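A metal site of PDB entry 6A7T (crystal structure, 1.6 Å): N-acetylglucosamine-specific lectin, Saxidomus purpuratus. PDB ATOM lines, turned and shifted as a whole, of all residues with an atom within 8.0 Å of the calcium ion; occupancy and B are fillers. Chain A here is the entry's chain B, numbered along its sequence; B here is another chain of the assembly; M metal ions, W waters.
Water W1 lies within hydrogen-bond range of OD2 of Asp 156 (2.7 Å), OG1 of Thr 65 (2.9 Å) and OE2 of Glu 67 (3.2 Å).
The calcium ion is bound by O of Thr 65 (2.3 Å), OE1 of Glu 67 (2.3 Å), water W2 (2.4 Å), OE2 of Glu 71 (2.4 Å), OE2 of Glu 154 (2.4 Å), water W1 (2.5 Å), OE1 of Glu 71 (2.8 Å) and OE1 of Glu 154 (2.8 Å).
Four residues have an atom within 4 Å of the calcium ion: Thr 65, Glu 67, Glu 71 and Glu 154.
The side-chain hydroxyl (OH) of Tyr 40 sits close to the side-chain carboxylate (OE2) of Glu 71, 2.6 Å away. N of Glu 71 sits at hydrogen-bond distance from SG of Cys 68. The side-chain carboxylate (OE2) of Glu 154 lies close to the side-chain hydroxyl (OG) of Ser 38, 2.6 Å away. SG of Cys 23 of chain B forms a disulfide with SG of Cys 68 (2.1 Å).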
ATOM      1  N   PHE A  35      25.925  16.494 -10.007  1.00  0.00           N
ATOM      2  CA  PHE A  35      24.960  17.625 -10.025  1.00  0.00           C
ATOM      3  C   PHE A  35      24.748  18.079 -11.469  1.00  0.00           C
ATOM      4  O   PHE A  35      25.699  18.328 -12.209  1.00  0.00           O
ATOM      5  CB  PHE A  35      25.432  18.791  -9.162  1.00  0.00           C
ATOM      6  CG  PHE A  35      24.511  19.986  -9.230  1.00  0.00           C
ATOM      7  CD1 PHE A  35      23.405  20.079  -8.380  1.00  0.00           C
ATOM      8  CD2 PHE A  35      24.668  20.944 -10.226  1.00  0.00           C
ATOM      9  CE1 PHE A  35      22.535  21.159  -8.480  1.00  0.00           C
ATOM     10  CE2 PHE A  35      23.787  22.011 -10.332  1.00  0.00           C
ATOM     11  CZ  PHE A  35      22.702  22.108  -9.472  1.00  0.00           C
ATOM     12  N   GLY A  36      23.477  18.275 -11.865  1.00  0.00           N
ATOM     13  CA  GLY A  36      23.156  18.952 -13.120  1.00  0.00           C
ATOM     14  C   GLY A  36      23.918  18.461 -14.354  1.00  0.00           C
ATOM     15  O   GLY A  36      24.485  19.237 -15.169  1.00  0.00           O
ATOM     16  N   GLY A  37      23.970  17.137 -14.524  1.00  0.00           N
ATOM     17  CA  GLY A  37      24.550  16.529 -15.714  1.00  0.00           C
ATOM     18  C   GLY A  37      26.083  16.520 -15.732  1.00  0.00           C
ATOM     19  O   GLY A  37      26.696  16.273 -16.757  1.00  0.00           O
ATOM     20  N   SER A  38      26.696  16.839 -14.593  1.00  0.00           N
ATOM     21  CA  SER A  38      28.140  16.843 -14.445  1.00  0.00           C
ATOM     22  C   SER A  38      28.553  16.037 -13.226  1.00  0.00           C
ATOM     23  O   SER A  38      27.850  15.896 -12.237  1.00  0.00           O
ATOM     24  CB  SER A  38      28.702  18.255 -14.331  1.00  0.00           C
ATOM     25  OG  SER A  38      28.751  18.908 -15.589  1.00  0.00           O
ATOM     26  N   TYR A  40      31.752  15.936 -10.419  1.00  0.00           N
ATOM     27  CA  TYR A  40      32.708  16.877  -9.847  1.00  0.00           C
ATOM     28  C   TYR A  40      33.644  16.184  -8.852  1.00  0.00           C
ATOM     29  O   TYR A  40      33.195  15.370  -7.992  1.00  0.00           O
ATOM     30  CB  TYR A  40      31.974  18.010  -9.105  1.00  0.00           C
ATOM     31  CG  TYR A  40      31.031  18.823  -9.957  1.00  0.00           C
ATOM     32  CD1 TYR A  40      29.720  18.424 -10.191  1.00  0.00           C
ATOM     33  CD2 TYR A  40      31.459  19.973 -10.566  1.00  0.00           C
ATOM     34  CE1 TYR A  40      28.853  19.164 -10.983  1.00  0.00           C
ATOM     35  CE2 TYR A  40      30.614  20.731 -11.366  1.00  0.00           C
ATOM     36  CZ  TYR A  40      29.301  20.327 -11.586  1.00  0.00           C
ATOM     37  OH  TYR A  40      28.475  21.066 -12.376  1.00  0.00           O
ATOM     38  N   LEU A  63      39.421  21.325 -15.072  1.00  0.00           N
ATOM     39  CA  LEU A  63      39.011  22.228 -14.021  1.00  0.00           C
ATOM     40  C   LEU A  63      37.608  22.762 -14.337  1.00  0.00           C
ATOM     41  O   LEU A  63      37.259  23.051 -15.502  1.00  0.00           O
ATOM     42  CB  LEU A  63      39.991  23.397 -13.883  1.00  0.00           C
ATOM     43  CG  LEU A  63      41.336  23.111 -13.199  1.00  0.00           C
ATOM     44  CD1 LEU A  63      42.303  24.246 -13.400  1.00  0.00           C
ATOM     45  CD2 LEU A  63      41.187  22.822 -11.706  1.00  0.00           C
ATOM     46  N   VAL A  64      36.793  22.937 -13.289  1.00  0.00           N
ATOM     47  CA  VAL A  64      35.370  23.192 -13.423  1.00  0.00           C
ATOM     48  C   VAL A  64      35.154  24.518 -14.145  1.00  0.00           C
ATOM     49  O   VAL A  64      35.920  25.503 -13.966  1.00  0.00           O
ATOM     50  CB  VAL A  64      34.698  23.146 -12.057  1.00  0.00           C
ATOM     51  CG1 VAL A  64      35.247  24.230 -11.152  1.00  0.00           C
ATOM     52  CG2 VAL A  64      33.192  23.298 -12.158  1.00  0.00           C
ATOM     53  N   THR A  65      34.107  24.523 -15.015  1.00  0.00           N
ATOM     54  CA  THR A  65      33.608  25.714 -15.688  1.00  0.00           C
ATOM     55  C   THR A  65      32.172  25.900 -15.206  1.00  0.00           C
ATOM     56  O   THR A  65      31.458  24.909 -15.060  1.00  0.00           O
ATOM     57  CB  THR A  65      33.757  25.610 -17.221  1.00  0.00           C
ATOM     58  OG1 THR A  65      32.916  24.569 -17.719  1.00  0.00           O
ATOM     59  CG2 THR A  65      35.180  25.369 -17.656  1.00  0.00           C
ATOM     60  N   VAL A  66      31.783  27.123 -14.919  1.00  0.00           N
ATOM     61  CA  VAL A  66      30.526  27.351 -14.215  1.00  0.00           C
ATOM     62  C   VAL A  66      29.585  28.179 -15.107  1.00  0.00           C
ATOM     63  O   VAL A  66      29.800  29.396 -15.273  1.00  0.00           O
ATOM     64  CB  VAL A  66      30.790  28.059 -12.875  1.00  0.00           C
ATOM     65  CG1 VAL A  66      29.528  28.329 -12.081  1.00  0.00           C
ATOM     66  CG2 VAL A  66      31.803  27.290 -12.018  1.00  0.00           C
ATOM     67  N   GLU A  67      28.602  27.495 -15.723  1.00  0.00           N
ATOM     68  CA  GLU A  67      27.810  28.101 -16.802  1.00  0.00           C
ATOM     69  C   GLU A  67      26.553  28.754 -16.251  1.00  0.00           C
ATOM     70  O   GLU A  67      25.954  29.536 -16.983  1.00  0.00           O
ATOM     71  CB  GLU A  67      27.479  27.040 -17.861  1.00  0.00           C
ATOM     72  CG  GLU A  67      28.673  26.740 -18.700  1.00  0.00           C
ATOM     73  CD  GLU A  67      29.649  25.730 -18.130  1.00  0.00           C
ATOM     74  OE1 GLU A  67      29.228  24.959 -17.222  1.00  0.00           O
ATOM     75  OE2 GLU A  67      30.741  25.597 -18.731  1.00  0.00           O
ATOM     76  N   CYS A  68      26.167  28.488 -15.012  1.00  0.00           N
ATOM     77  CA  CYS A  68      24.911  29.022 -14.504  1.00  0.00           C
ATOM     78  C   CYS A  68      24.914  29.153 -12.999  1.00  0.00           C
ATOM     79  O   CYS A  68      25.754  28.536 -12.276  1.00  0.00           O
ATOM     80  CB  CYS A  68      23.726  28.135 -14.904  1.00  0.00           C
ATOM     81  SG  CYS A  68      23.822  26.457 -14.213  1.00  0.00           S
ATOM     82  N   GLU A  71      24.693  25.893 -10.811  1.00  0.00           N
ATOM     83  CA  GLU A  71      25.934  25.160 -10.676  1.00  0.00           C
ATOM     84  C   GLU A  71      26.815  25.902  -9.630  1.00  0.00           C
ATOM     85  O   GLU A  71      27.429  25.309  -8.796  1.00  0.00           O
ATOM     86  CB  GLU A  71      26.616  25.085 -12.041  1.00  0.00           C
ATOM     87  CG  GLU A  71      27.873  24.253 -12.046  1.00  0.00           C
ATOM     88  CD  GLU A  71      28.514  24.074 -13.399  1.00  0.00           C
ATOM     89  OE1 GLU A  71      28.218  24.845 -14.375  1.00  0.00           O
ATOM     90  OE2 GLU A  71      29.355  23.206 -13.485  1.00  0.00           O
ATOM     91  N   ASP A  72      26.848  27.230  -9.756  1.00  0.00           N
ATOM     92  CA  ASP A  72      27.554  28.083  -8.791  1.00  0.00           C
ATOM     93  C   ASP A  72      27.019  27.785  -7.391  1.00  0.00           C
ATOM     94  O   ASP A  72      27.780  27.631  -6.455  1.00  0.00           O
ATOM     95  CB  ASP A  72      27.368  29.553  -9.126  1.00  0.00           C
ATOM     96  CG  ASP A  72      28.054  30.513  -8.168  1.00  0.00           C
ATOM     97  OD1 ASP A  72      29.280  30.587  -8.241  1.00  0.00           O
ATOM     98  OD2 ASP A  72      27.340  31.240  -7.448  1.00  0.00           O
ATOM     99  N   ILE A  75      28.163  24.391  -6.054  1.00  0.00           N
ATOM    100  CA  ILE A  75      29.594  24.382  -5.648  1.00  0.00           C
ATOM    101  C   ILE A  75      29.675  25.053  -4.256  1.00  0.00           C
ATOM    102  O   ILE A  75      30.345  24.560  -3.323  1.00  0.00           O
ATOM    103  CB  ILE A  75      30.464  25.076  -6.719  1.00  0.00           C
ATOM    104  CG1 ILE A  75      30.595  24.211  -7.967  1.00  0.00           C
ATOM    105  CG2 ILE A  75      31.819  25.496  -6.151  1.00  0.00           C
ATOM    106  CD1 ILE A  75      31.083  24.937  -9.182  1.00  0.00           C
ATOM    107  N   TRP A 103      36.814  30.791 -19.647  1.00  0.00           N
ATOM    108  CA  TRP A 103      37.040  29.438 -19.320  1.00  0.00           C
ATOM    109  C   TRP A 103      38.164  28.880 -20.198  1.00  0.00           C
ATOM    110  O   TRP A 103      38.384  29.375 -21.286  1.00  0.00           O
ATOM    111  CB  TRP A 103      35.770  28.596 -19.436  1.00  0.00           C
ATOM    112  CG  TRP A 103      34.658  29.141 -18.607  1.00  0.00           C
ATOM    113  CD1 TRP A 103      33.462  29.638 -19.039  1.00  0.00           C
ATOM    114  CD2 TRP A 103      34.594  29.212 -17.165  1.00  0.00           C
ATOM    115  NE1 TRP A 103      32.678  30.046 -17.987  1.00  0.00           N
ATOM    116  CE2 TRP A 103      33.357  29.796 -16.813  1.00  0.00           C
ATOM    117  CE3 TRP A 103      35.480  28.876 -16.140  1.00  0.00           C
ATOM    118  CZ2 TRP A 103      32.980  30.077 -15.506  1.00  0.00           C
ATOM    119  CZ3 TRP A 103      35.093  29.109 -14.844  1.00  0.00           C
ATOM    120  CH2 TRP A 103      33.889  29.707 -14.530  1.00  0.00           C
ATOM    121  N   GLU A 154      35.803  18.677 -13.158  1.00  0.00           N
ATOM    122  CA  GLU A 154      34.451  18.481 -13.742  1.00  0.00           C
ATOM    123  C   GLU A 154      34.570  17.562 -14.965  1.00  0.00           C
ATOM    124  O   GLU A 154      35.395  17.773 -15.794  1.00  0.00           O
ATOM    125  CB  GLU A 154      33.839  19.812 -14.166  1.00  0.00           C
ATOM    126  CG  GLU A 154      32.392  19.671 -14.658  1.00  0.00           C
ATOM    127  CD  GLU A 154      31.702  20.947 -15.137  1.00  0.00           C
ATOM    128  OE1 GLU A 154      32.428  21.979 -15.313  1.00  0.00           O
ATOM    129  OE2 GLU A 154      30.472  20.909 -15.368  1.00  0.00           O
ATOM    130  N   ILE A 155      33.685  16.546 -15.003  1.00  0.00           N
ATOM    131  CA  ILE A 155      33.384  15.758 -16.209  1.00  0.00           C
ATOM    132  C   ILE A 155      31.954  16.133 -16.608  1.00  0.00           C
ATOM    133  O   ILE A 155      31.059  15.945 -15.782  1.00  0.00           O
ATOM    134  CB  ILE A 155      33.480  14.267 -15.902  1.00  0.00           C
ATOM    135  CG1 ILE A 155      34.912  13.839 -15.568  1.00  0.00           C
ATOM    136  CG2 ILE A 155      32.934  13.450 -17.041  1.00  0.00           C
ATOM    137  CD1 ILE A 155      34.991  12.453 -14.913  1.00  0.00           C
ATOM    138  N   ASP A 156      31.760  16.665 -17.833  1.00  0.00           N
ATOM    139  CA  ASP A 156      30.411  17.112 -18.216  1.00  0.00           C
ATOM    140  C   ASP A 156      29.868  16.320 -19.421  1.00  0.00           C
ATOM    141  O   ASP A 156      28.726  16.546 -19.770  1.00  0.00           O
ATOM    142  CB  ASP A 156      30.340  18.627 -18.445  1.00  0.00           C
ATOM    143  CG  ASP A 156      31.086  19.160 -19.635  1.00  0.00           C
ATOM    144  OD1 ASP A 156      31.582  18.337 -20.410  1.00  0.00           O
ATOM    145  OD2 ASP A 156      31.219  20.407 -19.763  1.00  0.00           O
ATOM    146  N   CYS B  23      21.525  26.493 -17.607  1.00  0.00           N
ATOM    147  CA  CYS B  23      22.539  25.497 -17.361  1.00  0.00           C
ATOM    148  C   CYS B  23      22.659  24.610 -18.611  1.00  0.00           C
ATOM    149  O   CYS B  23      21.738  24.447 -19.408  1.00  0.00           O
ATOM    150  CB  CYS B  23      22.260  24.640 -16.131  1.00  0.00           C
ATOM    151  SG  CYS B  23      22.005  25.585 -14.595  1.00  0.00           S
ATOM    152  N   LYS B  24      23.828  24.026 -18.802  1.00  0.00           N
ATOM    153  CA  LYS B  24      24.095  23.204 -19.974  1.00  0.00           C
ATOM    154  C   LYS B  24      23.116  22.027 -20.152  1.00  0.00           C
ATOM    155  O   LYS B  24      22.843  21.603 -21.282  1.00  0.00           O
ATOM    156  CB  LYS B  24      25.498  22.596 -19.867  1.00  0.00           C
ATOM    157  CG  LYS B  24      26.613  23.543 -20.226  1.00  0.00           C
ATOM    158  CD  LYS B  24      27.946  22.857 -20.318  1.00  0.00           C
ATOM    159  CE  LYS B  24      28.092  21.909 -21.483  1.00  0.00           C
ATOM    160  NZ  LYS B  24      29.532  21.588 -21.682  1.00  0.00           N
ATOM    161  N   TRP B  33      21.511  23.397 -26.299  1.00  0.00           N
ATOM    162  CA  TRP B  33      22.228  24.436 -25.552  1.00  0.00           C
ATOM    163  C   TRP B  33      23.423  24.962 -26.342  1.00  0.00           C
ATOM    164  O   TRP B  33      24.171  24.182 -26.938  1.00  0.00           O
ATOM    165  CB  TRP B  33      22.707  23.864 -24.228  1.00  0.00           C
ATOM    166  CG  TRP B  33      23.283  24.869 -23.275  1.00  0.00           C
ATOM    167  CD1 TRP B  33      22.577  25.544 -22.331  1.00  0.00           C
ATOM    168  CD2 TRP B  33      24.652  25.318 -23.171  1.00  0.00           C
ATOM    169  NE1 TRP B  33      23.425  26.337 -21.608  1.00  0.00           N
ATOM    170  CE2 TRP B  33      24.691  26.222 -22.087  1.00  0.00           C
ATOM    171  CE3 TRP B  33      25.846  24.985 -23.818  1.00  0.00           C
ATOM    172  CZ2 TRP B  33      25.855  26.881 -21.683  1.00  0.00           C
ATOM    173  CZ3 TRP B  33      27.009  25.626 -23.406  1.00  0.00           C
ATOM    174  CH2 TRP B  33      27.011  26.573 -22.376  1.00  0.00           C
HETATM  175 CA    CA M   1      29.996  23.260 -15.793  1.00  0.00          CA
HETATM  176  O   HOH W   1      30.899  22.460 -18.025  1.00  0.00           O
HETATM  177  O   HOH W   2      27.855  22.322 -16.316  1.00  0.00           O
